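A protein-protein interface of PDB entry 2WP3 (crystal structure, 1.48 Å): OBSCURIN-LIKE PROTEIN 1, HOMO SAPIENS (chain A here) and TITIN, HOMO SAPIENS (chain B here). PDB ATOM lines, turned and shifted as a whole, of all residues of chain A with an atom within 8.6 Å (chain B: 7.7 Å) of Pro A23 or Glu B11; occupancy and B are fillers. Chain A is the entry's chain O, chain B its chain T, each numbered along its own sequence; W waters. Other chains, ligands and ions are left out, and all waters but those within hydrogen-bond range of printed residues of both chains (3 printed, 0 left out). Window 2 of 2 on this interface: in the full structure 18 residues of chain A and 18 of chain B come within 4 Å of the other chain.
NH1 of Arg A22 is in salt-bridge range of OD1 of Asp B63 (3.0 Å).
Water W1 lies within hydrogen-bond range of the backbone carbonyl oxygen (O) of Ala B12, the backbone NH (N) of Ala B30 and the backbone carbonyl oxygen (O) of Ala A99. Water W2 lies within hydrogen-bond range of O of Ala B12 (2.8 Å) and N of Ala A99 (2.8 Å). Water W3 bridges O of Phe B31 and NH2 of Arg A22.
Among the printed residues, pairs that only touch across the chains: Arg A22 with Ala B30, Pro A23 with Glu B11, Ala A99 with Ala B12, Ala A100 with Ala B12, Phe A20 with Leu B64, Phe A20 with Ala B30, Ala A99 with Pro B14, Ala A99 with Leu B13, Val A84 with Ala B12, Phe A20 with Cys B29 and Ala A101 with Ala B12.
Printed residues of chain A that touch a printed residue of chain B: Phe A20, Arg A22, Pro A23, Val A84, Ala A99, Ala A100 and Ala A101. Of the 17 printed residues of chain B, 8 touch a printed residue of chain A. Hydrophobic or aromatic side chains of chain B that line the printed part of chain A: Ala B12, Pro B14, Ala B30 and Leu B64. Among the printed residues, 12 pairs touch across the chains. Among the printed residues, Asp or Glu carboxylates within 4 Å of a Lys or Arg side-chain nitrogen of the other chain: Arg A22 with Asp B63 (3.0 Å).
O of Asp B63 sits at hydrogen-bond distance from N of Phe B31, at 3.1 Å. N of Val A24 sits at hydrogen-bond distance from O of Ala A101, at 3.2 Å. The backbone carbonyl oxygen (O) of Ala B12 lies within hydrogen-bond range of the side-chain sulfur (SG) of Cys B29, at 3.4 Å. The backbone carbonyl oxygen (O) of Ala B30 sits at hydrogen-bond distance from the backbone NH (N) of Glu B11 (2.9 Å).
Printed residues of chain B within 4 Å of Pro A23: Glu B11. Printed residues of chain A within 4 Å of Glu B11: Pro A23. Printed residues of chain B within 4 Å of Phe A20: Cys B29, Ala B30 and Leu B64. Printed residues of chain B within 4 Å of Ala A100: Ala B12. Leu B84 touches none of the printed residues of chain A. The nearest printed residue of chain A that does not touch Glu B11 is Ala A99 (5.5 Å).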
ATOM      1  N   PHE A  20      -6.237 -20.786 -12.002  1.00  0.00           N
ATOM      2  CA  PHE A  20      -4.873 -20.443 -11.639  1.00  0.00           C
ATOM      3  C   PHE A  20      -4.811 -20.212 -10.133  1.00  0.00           C
ATOM      4  O   PHE A  20      -5.753 -19.694  -9.535  1.00  0.00           O
ATOM      5  CB  PHE A  20      -4.430 -19.184 -12.419  1.00  0.00           C
ATOM      6  CG  PHE A  20      -2.973 -18.779 -12.166  1.00  0.00           C
ATOM      7  CD1 PHE A  20      -1.974 -19.248 -12.982  1.00  0.00           C
ATOM      8  CD2 PHE A  20      -2.636 -17.932 -11.121  1.00  0.00           C
ATOM      9  CE1 PHE A  20      -0.614 -18.911 -12.754  1.00  0.00           C
ATOM     10  CE2 PHE A  20      -1.301 -17.579 -10.876  1.00  0.00           C
ATOM     11  CZ  PHE A  20      -0.283 -18.057 -11.702  1.00  0.00           C
ATOM     12  N   PRO A  21      -3.693 -20.632  -9.494  1.00  0.00           N
ATOM     13  CA  PRO A  21      -3.588 -20.512  -8.048  1.00  0.00           C
ATOM     14  C   PRO A  21      -3.325 -19.103  -7.640  1.00  0.00           C
ATOM     15  O   PRO A  21      -2.234 -18.563  -7.938  1.00  0.00           O
ATOM     16  CB  PRO A  21      -2.363 -21.368  -7.704  1.00  0.00           C
ATOM     17  CG  PRO A  21      -1.568 -21.418  -8.902  1.00  0.00           C
ATOM     18  CD  PRO A  21      -2.541 -21.353 -10.057  1.00  0.00           C
ATOM     19  N   ARG A  22      -4.293 -18.501  -6.971  1.00  0.00           N
ATOM     20  CA  ARG A  22      -4.111 -17.120  -6.517  1.00  0.00           C
ATOM     21  C   ARG A  22      -3.395 -17.034  -5.157  1.00  0.00           C
ATOM     22  O   ARG A  22      -3.359 -17.992  -4.388  1.00  0.00           O
ATOM     23  CB  ARG A  22      -5.446 -16.382  -6.565  1.00  0.00           C
ATOM     24  CG  ARG A  22      -6.040 -16.336  -8.002  1.00  0.00           C
ATOM     25  CD  ARG A  22      -5.326 -15.362  -9.016  1.00  0.00           C
ATOM     26  NE  ARG A  22      -5.899 -15.493 -10.372  1.00  0.00           N
ATOM     27  CZ  ARG A  22      -5.636 -14.737 -11.441  1.00  0.00           C
ATOM     28  NH1 ARG A  22      -6.246 -15.006 -12.588  1.00  0.00           N
ATOM     29  NH2 ARG A  22      -4.806 -13.696 -11.389  1.00  0.00           N
ATOM     30  N   PRO A  23      -2.781 -15.882  -4.871  1.00  0.00           N
ATOM     31  CA  PRO A  23      -2.104 -15.772  -3.584  1.00  0.00           C
ATOM     32  C   PRO A  23      -3.028 -15.860  -2.413  1.00  0.00           C
ATOM     33  O   PRO A  23      -4.229 -15.567  -2.526  1.00  0.00           O
ATOM     34  CB  PRO A  23      -1.429 -14.393  -3.643  1.00  0.00           C
ATOM     35  CG  PRO A  23      -2.150 -13.664  -4.685  1.00  0.00           C
ATOM     36  CD  PRO A  23      -2.547 -14.679  -5.701  1.00  0.00           C
ATOM     37  N   VAL A  24      -2.435 -16.263  -1.283  1.00  0.00           N
ATOM     38  CA  VAL A  24      -3.183 -16.440  -0.040  1.00  0.00           C
ATOM     39  C   VAL A  24      -2.497 -15.546   0.993  1.00  0.00           C
ATOM     40  O   VAL A  24      -1.245 -15.536   1.098  1.00  0.00           O
ATOM     41  CB  VAL A  24      -3.331 -17.947   0.345  1.00  0.00           C
ATOM     42  CG1 VAL A  24      -4.143 -18.654  -0.716  1.00  0.00           C
ATOM     43  CG2 VAL A  24      -2.034 -18.625   0.461  1.00  0.00           C
ATOM     44  N   ARG A  25      -3.305 -14.751   1.688  1.00  0.00           N
ATOM     45  CA  ARG A  25      -2.828 -13.935   2.795  1.00  0.00           C
ATOM     46  C   ARG A  25      -3.603 -14.492   3.987  1.00  0.00           C
ATOM     47  O   ARG A  25      -4.819 -14.361   4.008  1.00  0.00           O
ATOM     48  CB  ARG A  25      -3.197 -12.452   2.627  1.00  0.00           C
ATOM     49  CG  ARG A  25      -2.813 -11.861   1.278  1.00  0.00           C
ATOM     50  CD  ARG A  25      -2.899 -10.357   1.267  1.00  0.00           C
ATOM     51  NE  ARG A  25      -1.551  -9.820   1.483  1.00  0.00           N
ATOM     52  CZ  ARG A  25      -1.195  -8.954   2.432  1.00  0.00           C
ATOM     53  NH1 ARG A  25      -2.086  -8.443   3.286  1.00  0.00           N
ATOM     54  NH2 ARG A  25       0.075  -8.571   2.516  1.00  0.00           N
ATOM     55  N   VAL A  26      -2.910 -14.966   4.995  1.00  0.00           N
ATOM     56  CA  VAL A  26      -3.496 -15.739   6.090  1.00  0.00           C
ATOM     57  C   VAL A  26      -2.887 -15.343   7.436  1.00  0.00           C
ATOM     58  O   VAL A  26      -1.689 -15.104   7.549  1.00  0.00           O
ATOM     59  CB  VAL A  26      -3.256 -17.284   5.825  1.00  0.00           C
ATOM     60  CG1 VAL A  26      -1.815 -17.667   5.750  1.00  0.00           C
ATOM     61  CG2 VAL A  26      -3.976 -18.162   6.841  1.00  0.00           C
ATOM     62  N   ALA A  32      -4.650 -22.531   5.403  1.00  0.00           N
ATOM     63  CA  ALA A  32      -4.402 -21.861   4.121  1.00  0.00           C
ATOM     64  C   ALA A  32      -4.452 -22.908   3.015  1.00  0.00           C
ATOM     65  O   ALA A  32      -3.934 -23.997   3.201  1.00  0.00           O
ATOM     66  CB  ALA A  32      -3.034 -21.170   4.096  1.00  0.00           C
ATOM     67  N   GLU A  33      -5.024 -22.568   1.864  1.00  0.00           N
ATOM     68  CA  GLU A  33      -4.974 -23.468   0.719  1.00  0.00           C
ATOM     69  C   GLU A  33      -4.751 -22.746  -0.585  1.00  0.00           C
ATOM     70  O   GLU A  33      -5.418 -21.763  -0.886  1.00  0.00           O
ATOM     71  CB  GLU A  33      -6.228 -24.372   0.520  1.00  0.00           C
ATOM     72  CG  GLU A  33      -5.961 -25.638  -0.388  1.00  0.00           C
ATOM     73  CD  GLU A  33      -7.058 -26.706  -0.390  1.00  0.00           C
ATOM     74  OE1 GLU A  33      -7.959 -26.711   0.499  1.00  0.00           O
ATOM     75  OE2 GLU A  33      -7.034 -27.554  -1.307  1.00  0.00           O
ATOM     76  N   LEU A  34      -3.800 -23.268  -1.326  1.00  0.00           N
ATOM     77  CA  LEU A  34      -3.586 -22.883  -2.725  1.00  0.00           C
ATOM     78  C   LEU A  34      -4.309 -23.904  -3.562  1.00  0.00           C
ATOM     79  O   LEU A  34      -4.282 -25.097  -3.235  1.00  0.00           O
ATOM     80  CB  LEU A  34      -2.109 -22.867  -3.089  1.00  0.00           C
ATOM     81  CG  LEU A  34      -1.154 -21.961  -2.299  1.00  0.00           C
ATOM     82  CD1 LEU A  34       0.322 -22.262  -2.599  1.00  0.00           C
ATOM     83  CD2 LEU A  34      -1.579 -20.475  -2.488  1.00  0.00           C
ATOM     84  N   LYS A  35      -4.964 -23.420  -4.615  1.00  0.00           N
ATOM     85  CA  LYS A  35      -5.924 -24.205  -5.373  1.00  0.00           C
ATOM     86  C   LYS A  35      -5.845 -23.946  -6.875  1.00  0.00           C
ATOM     87  O   LYS A  35      -5.707 -22.806  -7.316  1.00  0.00           O
ATOM     88  CB  LYS A  35      -7.331 -23.889  -4.881  1.00  0.00           C
ATOM     89  CG  LYS A  35      -7.529 -24.079  -3.378  1.00  0.00           C
ATOM     90  CD  LYS A  35      -8.894 -23.541  -2.988  1.00  0.00           C
ATOM     91  CE  LYS A  35      -9.379 -24.118  -1.667  1.00  0.00           C
ATOM     92  NZ  LYS A  35     -10.858 -23.964  -1.616  1.00  0.00           N
ATOM     93  N   GLY A  83       6.128 -17.568   1.541  1.00  0.00           N
ATOM     94  CA  GLY A  83       6.996 -17.683   0.359  1.00  0.00           C
ATOM     95  C   GLY A  83       6.263 -18.123  -0.878  1.00  0.00           C
ATOM     96  O   GLY A  83       5.021 -18.132  -0.914  1.00  0.00           O
ATOM     97  N   VAL A  84       7.058 -18.465  -1.900  1.00  0.00           N
ATOM     98  CA  VAL A  84       6.555 -18.825  -3.218  1.00  0.00           C
ATOM     99  C   VAL A  84       6.550 -20.336  -3.393  1.00  0.00           C
ATOM    100  O   VAL A  84       7.569 -21.006  -3.193  1.00  0.00           O
ATOM    101  CB  VAL A  84       7.376 -18.172  -4.349  1.00  0.00           C
ATOM    102  CG1 VAL A  84       6.913 -18.637  -5.705  1.00  0.00           C
ATOM    103  CG2 VAL A  84       7.287 -16.666  -4.235  1.00  0.00           C
ATOM    104  N   ALA A  99       3.226 -20.220 -10.303  1.00  0.00           N
ATOM    105  CA  ALA A  99       3.627 -19.912  -8.923  1.00  0.00           C
ATOM    106  C   ALA A  99       2.597 -19.080  -8.156  1.00  0.00           C
ATOM    107  O   ALA A  99       1.852 -18.314  -8.721  1.00  0.00           O
ATOM    108  CB  ALA A  99       4.989 -19.233  -8.886  1.00  0.00           C
ATOM    109  N   ALA A 100       2.557 -19.284  -6.838  1.00  0.00           N
ATOM    110  CA  ALA A 100       1.727 -18.463  -5.980  1.00  0.00           C
ATOM    111  C   ALA A 100       2.393 -18.270  -4.619  1.00  0.00           C
ATOM    112  O   ALA A 100       3.073 -19.167  -4.120  1.00  0.00           O
ATOM    113  CB  ALA A 100       0.336 -19.102  -5.827  1.00  0.00           C
ATOM    114  N   ALA A 101       2.198 -17.080  -4.033  1.00  0.00           N
ATOM    115  CA  ALA A 101       2.840 -16.686  -2.796  1.00  0.00           C
ATOM    116  C   ALA A 101       1.895 -16.829  -1.588  1.00  0.00           C
ATOM    117  O   ALA A 101       0.723 -16.481  -1.739  1.00  0.00           O
ATOM    118  CB  ALA A 101       3.269 -15.208  -2.858  1.00  0.00           C
ATOM    119  N   VAL A 102       2.407 -17.345  -0.489  1.00  0.00           N
ATOM    120  CA  VAL A 102       1.677 -17.379   0.779  1.00  0.00           C
ATOM    121  C   VAL A 102       2.279 -16.232   1.604  1.00  0.00           C
ATOM    122  O   VAL A 102       3.496 -16.198   1.810  1.00  0.00           O
ATOM    123  CB  VAL A 102       1.827 -18.708   1.481  1.00  0.00           C
ATOM    124  CG1 VAL A 102       1.171 -18.710   2.852  1.00  0.00           C
ATOM    125  CG2 VAL A 102       1.253 -19.822   0.601  1.00  0.00           C
ATOM    126  N   THR A 103       1.435 -15.314   2.109  1.00  0.00           N
ATOM    127  CA  THR A 103       1.874 -14.277   3.065  1.00  0.00           C
ATOM    128  C   THR A 103       1.225 -14.622   4.426  1.00  0.00           C
ATOM    129  O   THR A 103       0.052 -14.942   4.460  1.00  0.00           O
ATOM    130  CB  THR A 103       1.393 -12.888   2.625  1.00  0.00           C
ATOM    131  OG1 THR A 103       1.944 -12.565   1.338  1.00  0.00           O
ATOM    132  CG2 THR A 103       1.733 -11.779   3.640  1.00  0.00           C
ATOM    133  N   PRO B   8       2.008  -1.542 -11.187  1.00  0.00           N
ATOM    134  CA  PRO B   8       1.883  -2.976 -11.410  1.00  0.00           C
ATOM    135  C   PRO B   8       2.698  -3.864 -10.490  1.00  0.00           C
ATOM    136  O   PRO B   8       3.736  -3.433  -9.967  1.00  0.00           O
ATOM    137  CB  PRO B   8       2.350  -3.135 -12.865  1.00  0.00           C
ATOM    138  CG  PRO B   8       2.857  -1.860 -13.306  1.00  0.00           C
ATOM    139  CD  PRO B   8       2.900  -0.923 -12.167  1.00  0.00           C
ATOM    140  N   LYS B   9       2.202  -5.088 -10.282  1.00  0.00           N
ATOM    141  CA  LYS B   9       2.832  -6.053  -9.490  1.00  0.00           C
ATOM    142  C   LYS B   9       2.699  -7.419 -10.133  1.00  0.00           C
ATOM    143  O   LYS B   9       1.586  -7.889 -10.417  1.00  0.00           O
ATOM    144  CB  LYS B   9       2.163  -6.117  -8.119  1.00  0.00           C
ATOM    145  CG  LYS B   9       2.622  -7.313  -7.218  1.00  0.00           C
ATOM    146  CD  LYS B   9       4.044  -7.181  -6.735  1.00  0.00           C
ATOM    147  CE  LYS B   9       4.434  -8.392  -5.855  1.00  0.00           C
ATOM    148  NZ  LYS B   9       5.903  -8.363  -5.577  1.00  0.00           N
ATOM    149  N   ILE B  10       3.846  -8.029 -10.408  1.00  0.00           N
ATOM    150  CA  ILE B  10       3.920  -9.422 -10.806  1.00  0.00           C
ATOM    151  C   ILE B  10       3.789 -10.274  -9.576  1.00  0.00           C
ATOM    152  O   ILE B  10       4.605 -10.188  -8.650  1.00  0.00           O
ATOM    153  CB  ILE B  10       5.263  -9.745 -11.453  1.00  0.00           C
ATOM    154  CG1 ILE B  10       5.412  -8.910 -12.717  1.00  0.00           C
ATOM    155  CG2 ILE B  10       5.426 -11.284 -11.683  1.00  0.00           C
ATOM    156  CD1 ILE B  10       6.813  -8.911 -13.291  1.00  0.00           C
ATOM    157  N   GLU B  11       2.770 -11.114  -9.550  1.00  0.00           N
ATOM    158  CA  GLU B  11       2.708 -12.070  -8.475  1.00  0.00           C
ATOM    159  C   GLU B  11       3.843 -13.035  -8.692  1.00  0.00           C
ATOM    160  O   GLU B  11       4.855 -12.823  -9.366  1.00  0.00           O
ATOM    161  CB  GLU B  11       1.378 -12.836  -8.476  1.00  0.00           C
ATOM    162  CG  GLU B  11       0.154 -11.931  -8.596  1.00  0.00           C
ATOM    163  CD  GLU B  11      -0.524 -11.568  -7.292  1.00  0.00           C
ATOM    164  OE1 GLU B  11      -1.743 -11.293  -7.356  1.00  0.00           O
ATOM    165  OE2 GLU B  11       0.133 -11.539  -6.218  1.00  0.00           O
ATOM    166  N   ALA B  12       3.660 -14.173  -8.134  1.00  0.00           N
ATOM    167  CA  ALA B  12       4.752 -15.058  -8.085  1.00  0.00           C
ATOM    168  C   ALA B  12       5.132 -15.594  -9.508  1.00  0.00           C
ATOM    169  O   ALA B  12       4.246 -15.855 -10.311  1.00  0.00           O
ATOM    170  CB  ALA B  12       4.337 -16.096  -7.178  1.00  0.00           C
ATOM    171  N   LEU B  13       6.418 -15.807  -9.747  1.00  0.00           N
ATOM    172  CA  LEU B  13       6.892 -16.432 -10.989  1.00  0.00           C
ATOM    173  C   LEU B  13       7.961 -17.406 -10.610  1.00  0.00           C
ATOM    174  O   LEU B  13       8.769 -17.067  -9.767  1.00  0.00           O
ATOM    175  CB  LEU B  13       7.453 -15.347 -11.891  1.00  0.00           C
ATOM    176  CG  LEU B  13       7.868 -15.771 -13.309  1.00  0.00           C
ATOM    177  CD1 LEU B  13       6.642 -16.136 -14.203  1.00  0.00           C
ATOM    178  CD2 LEU B  13       8.686 -14.664 -14.007  1.00  0.00           C
ATOM    179  N   PRO B  14       7.969 -18.676 -11.147  1.00  0.00           N
ATOM    180  CA  PRO B  14       9.022 -19.572 -10.777  1.00  0.00           C
ATOM    181  C   PRO B  14      10.357 -18.961 -11.164  1.00  0.00           C
ATOM    182  O   PRO B  14      10.453 -18.285 -12.210  1.00  0.00           O
ATOM    183  CB  PRO B  14       8.758 -20.824 -11.661  1.00  0.00           C
ATOM    184  CG  PRO B  14       7.318 -20.757 -12.002  1.00  0.00           C
ATOM    185  CD  PRO B  14       7.016 -19.306 -12.095  1.00  0.00           C
ATOM    186  N   CYS B  29       1.292 -16.492 -15.166  1.00  0.00           N
ATOM    187  CA  CYS B  29       1.659 -15.587 -14.070  1.00  0.00           C
ATOM    188  C   CYS B  29       0.564 -14.536 -13.914  1.00  0.00           C
ATOM    189  O   CYS B  29       0.148 -13.901 -14.897  1.00  0.00           O
ATOM    190  CB  CYS B  29       3.008 -14.946 -14.361  1.00  0.00           C
ATOM    191  SG  CYS B  29       3.693 -13.946 -13.023  1.00  0.00           S
ATOM    192  N   ALA B  30       0.117 -14.371 -12.661  1.00  0.00           N
ATOM    193  CA  ALA B  30      -0.874 -13.353 -12.297  1.00  0.00           C
ATOM    194  C   ALA B  30      -0.222 -11.977 -12.011  1.00  0.00           C
ATOM    195  O   ALA B  30       0.958 -11.907 -11.651  1.00  0.00           O
ATOM    196  CB  ALA B  30      -1.684 -13.833 -11.048  1.00  0.00           C
ATOM    197  N   PHE B  31      -1.031 -10.941 -12.236  1.00  0.00           N
ATOM    198  CA  PHE B  31      -0.568  -9.607 -11.945  1.00  0.00           C
ATOM    199  C   PHE B  31      -1.688  -8.704 -11.544  1.00  0.00           C
ATOM    200  O   PHE B  31      -2.879  -8.973 -11.783  1.00  0.00           O
ATOM    201  CB  PHE B  31       0.227  -9.015 -13.127  1.00  0.00           C
ATOM    202  CG  PHE B  31      -0.541  -8.922 -14.408  1.00  0.00           C
ATOM    203  CD1 PHE B  31      -1.392  -7.855 -14.612  1.00  0.00           C
ATOM    204  CD2 PHE B  31      -0.468  -9.868 -15.435  1.00  0.00           C
ATOM    205  CE1 PHE B  31      -2.140  -7.714 -15.798  1.00  0.00           C
ATOM    206  CE2 PHE B  31      -1.226  -9.743 -16.597  1.00  0.00           C
ATOM    207  CZ  PHE B  31      -2.065  -8.711 -16.760  1.00  0.00           C
ATOM    208  N   THR B  32      -1.268  -7.600 -10.952  1.00  0.00           N
ATOM    209  CA  THR B  32      -2.190  -6.531 -10.629  1.00  0.00           C
ATOM    210  C   THR B  32      -1.702  -5.185 -11.161  1.00  0.00           C
ATOM    211  O   THR B  32      -0.547  -5.045 -11.550  1.00  0.00           O
ATOM    212  CB  THR B  32      -2.401  -6.415  -9.087  1.00  0.00           C
ATOM    213  OG1 THR B  32      -1.157  -6.135  -8.430  1.00  0.00           O
ATOM    214  CG2 THR B  32      -2.990  -7.751  -8.498  1.00  0.00           C
ATOM    215  N   ASP B  63      -5.668  -9.854 -15.823  1.00  0.00           N
ATOM    216  CA  ASP B  63      -4.886 -10.248 -14.632  1.00  0.00           C
ATOM    217  C   ASP B  63      -4.002 -11.511 -14.714  1.00  0.00           C
ATOM    218  O   ASP B  63      -3.537 -11.974 -13.701  1.00  0.00           O
ATOM    219  CB  ASP B  63      -5.886 -10.355 -13.445  1.00  0.00           C
ATOM    220  CG  ASP B  63      -6.887 -11.499 -13.624  1.00  0.00           C
ATOM    221  OD1 ASP B  63      -6.568 -12.509 -14.268  1.00  0.00           O
ATOM    222  OD2 ASP B  63      -8.014 -11.388 -13.082  1.00  0.00           O
ATOM    223  N   LEU B  64      -3.784 -12.050 -15.912  1.00  0.00           N
ATOM    224  CA  LEU B  64      -3.011 -13.223 -16.132  1.00  0.00           C
ATOM    225  C   LEU B  64      -2.303 -13.041 -17.485  1.00  0.00           C
ATOM    226  O   LEU B  64      -2.920 -12.427 -18.430  1.00  0.00           O
ATOM    227  CB  LEU B  64      -3.933 -14.458 -16.140  1.00  0.00           C
ATOM    228  CG  LEU B  64      -3.118 -15.727 -15.974  1.00  0.00           C
ATOM    229  CD1 LEU B  64      -2.484 -15.897 -14.575  1.00  0.00           C
ATOM    230  CD2 LEU B  64      -3.995 -16.918 -16.284  1.00  0.00           C
ATOM    231  N   LEU B  82       9.678 -11.093 -17.647  1.00  0.00           N
ATOM    232  CA  LEU B  82       8.340 -10.557 -17.735  1.00  0.00           C
ATOM    233  C   LEU B  82       8.404  -9.162 -17.125  1.00  0.00           C
ATOM    234  O   LEU B  82       8.818  -9.015 -15.978  1.00  0.00           O
ATOM    235  CB  LEU B  82       7.377 -11.433 -16.931  1.00  0.00           C
ATOM    236  CG  LEU B  82       5.972 -10.844 -16.738  1.00  0.00           C
ATOM    237  CD1 LEU B  82       5.239 -10.568 -18.072  1.00  0.00           C
ATOM    238  CD2 LEU B  82       5.153 -11.809 -15.850  1.00  0.00           C
ATOM    239  N   LEU B  84       6.064  -5.405 -16.597  1.00  0.00           N
ATOM    240  CA  LEU B  84       4.793  -4.754 -16.589  1.00  0.00           C
ATOM    241  C   LEU B  84       5.029  -3.241 -16.473  1.00  0.00           C
ATOM    242  O   LEU B  84       5.921  -2.812 -15.696  1.00  0.00           O
ATOM    243  CB  LEU B  84       4.002  -5.212 -15.370  1.00  0.00           C
ATOM    244  CG  LEU B  84       3.646  -6.673 -15.250  1.00  0.00           C
ATOM    245  CD1 LEU B  84       2.796  -6.932 -13.977  1.00  0.00           C
ATOM    246  CD2 LEU B  84       2.916  -7.214 -16.466  1.00  0.00           C
ATOM    247  N   ASP B  91       7.182  -3.159 -13.001  1.00  0.00           N
ATOM    248  CA  ASP B  91       7.714  -4.313 -12.271  1.00  0.00           C
ATOM    249  C   ASP B  91       8.327  -5.256 -13.280  1.00  0.00           C
ATOM    250  O   ASP B  91       7.961  -5.188 -14.456  1.00  0.00           O
ATOM    251  CB  ASP B  91       6.627  -5.015 -11.450  1.00  0.00           C
ATOM    252  CG  ASP B  91       7.190  -6.008 -10.378  1.00  0.00           C
ATOM    253  OD1 ASP B  91       8.385  -5.912  -9.969  1.00  0.00           O
ATOM    254  OD2 ASP B  91       6.361  -6.779  -9.801  1.00  0.00           O
ATOM    255  N   ALA B  93      10.306  -9.463 -13.409  1.00  0.00           N
ATOM    256  CA  ALA B  93      10.785 -10.707 -12.763  1.00  0.00           C
ATOM    257  C   ALA B  93      11.290 -11.613 -13.843  1.00  0.00           C
ATOM    258  O   ALA B  93      10.933 -11.435 -15.023  1.00  0.00           O
ATOM    259  CB  ALA B  93       9.612 -11.363 -12.025  1.00  0.00           C
HETATM  260  O   HOH W   1       1.512 -15.617 -10.325  1.00  0.00           O
HETATM  261  O   HOH W   2       3.849 -18.022 -12.006  1.00  0.00           O
HETATM  262  O   HOH W   3      -4.066 -10.988 -10.244  1.00  0.00           O
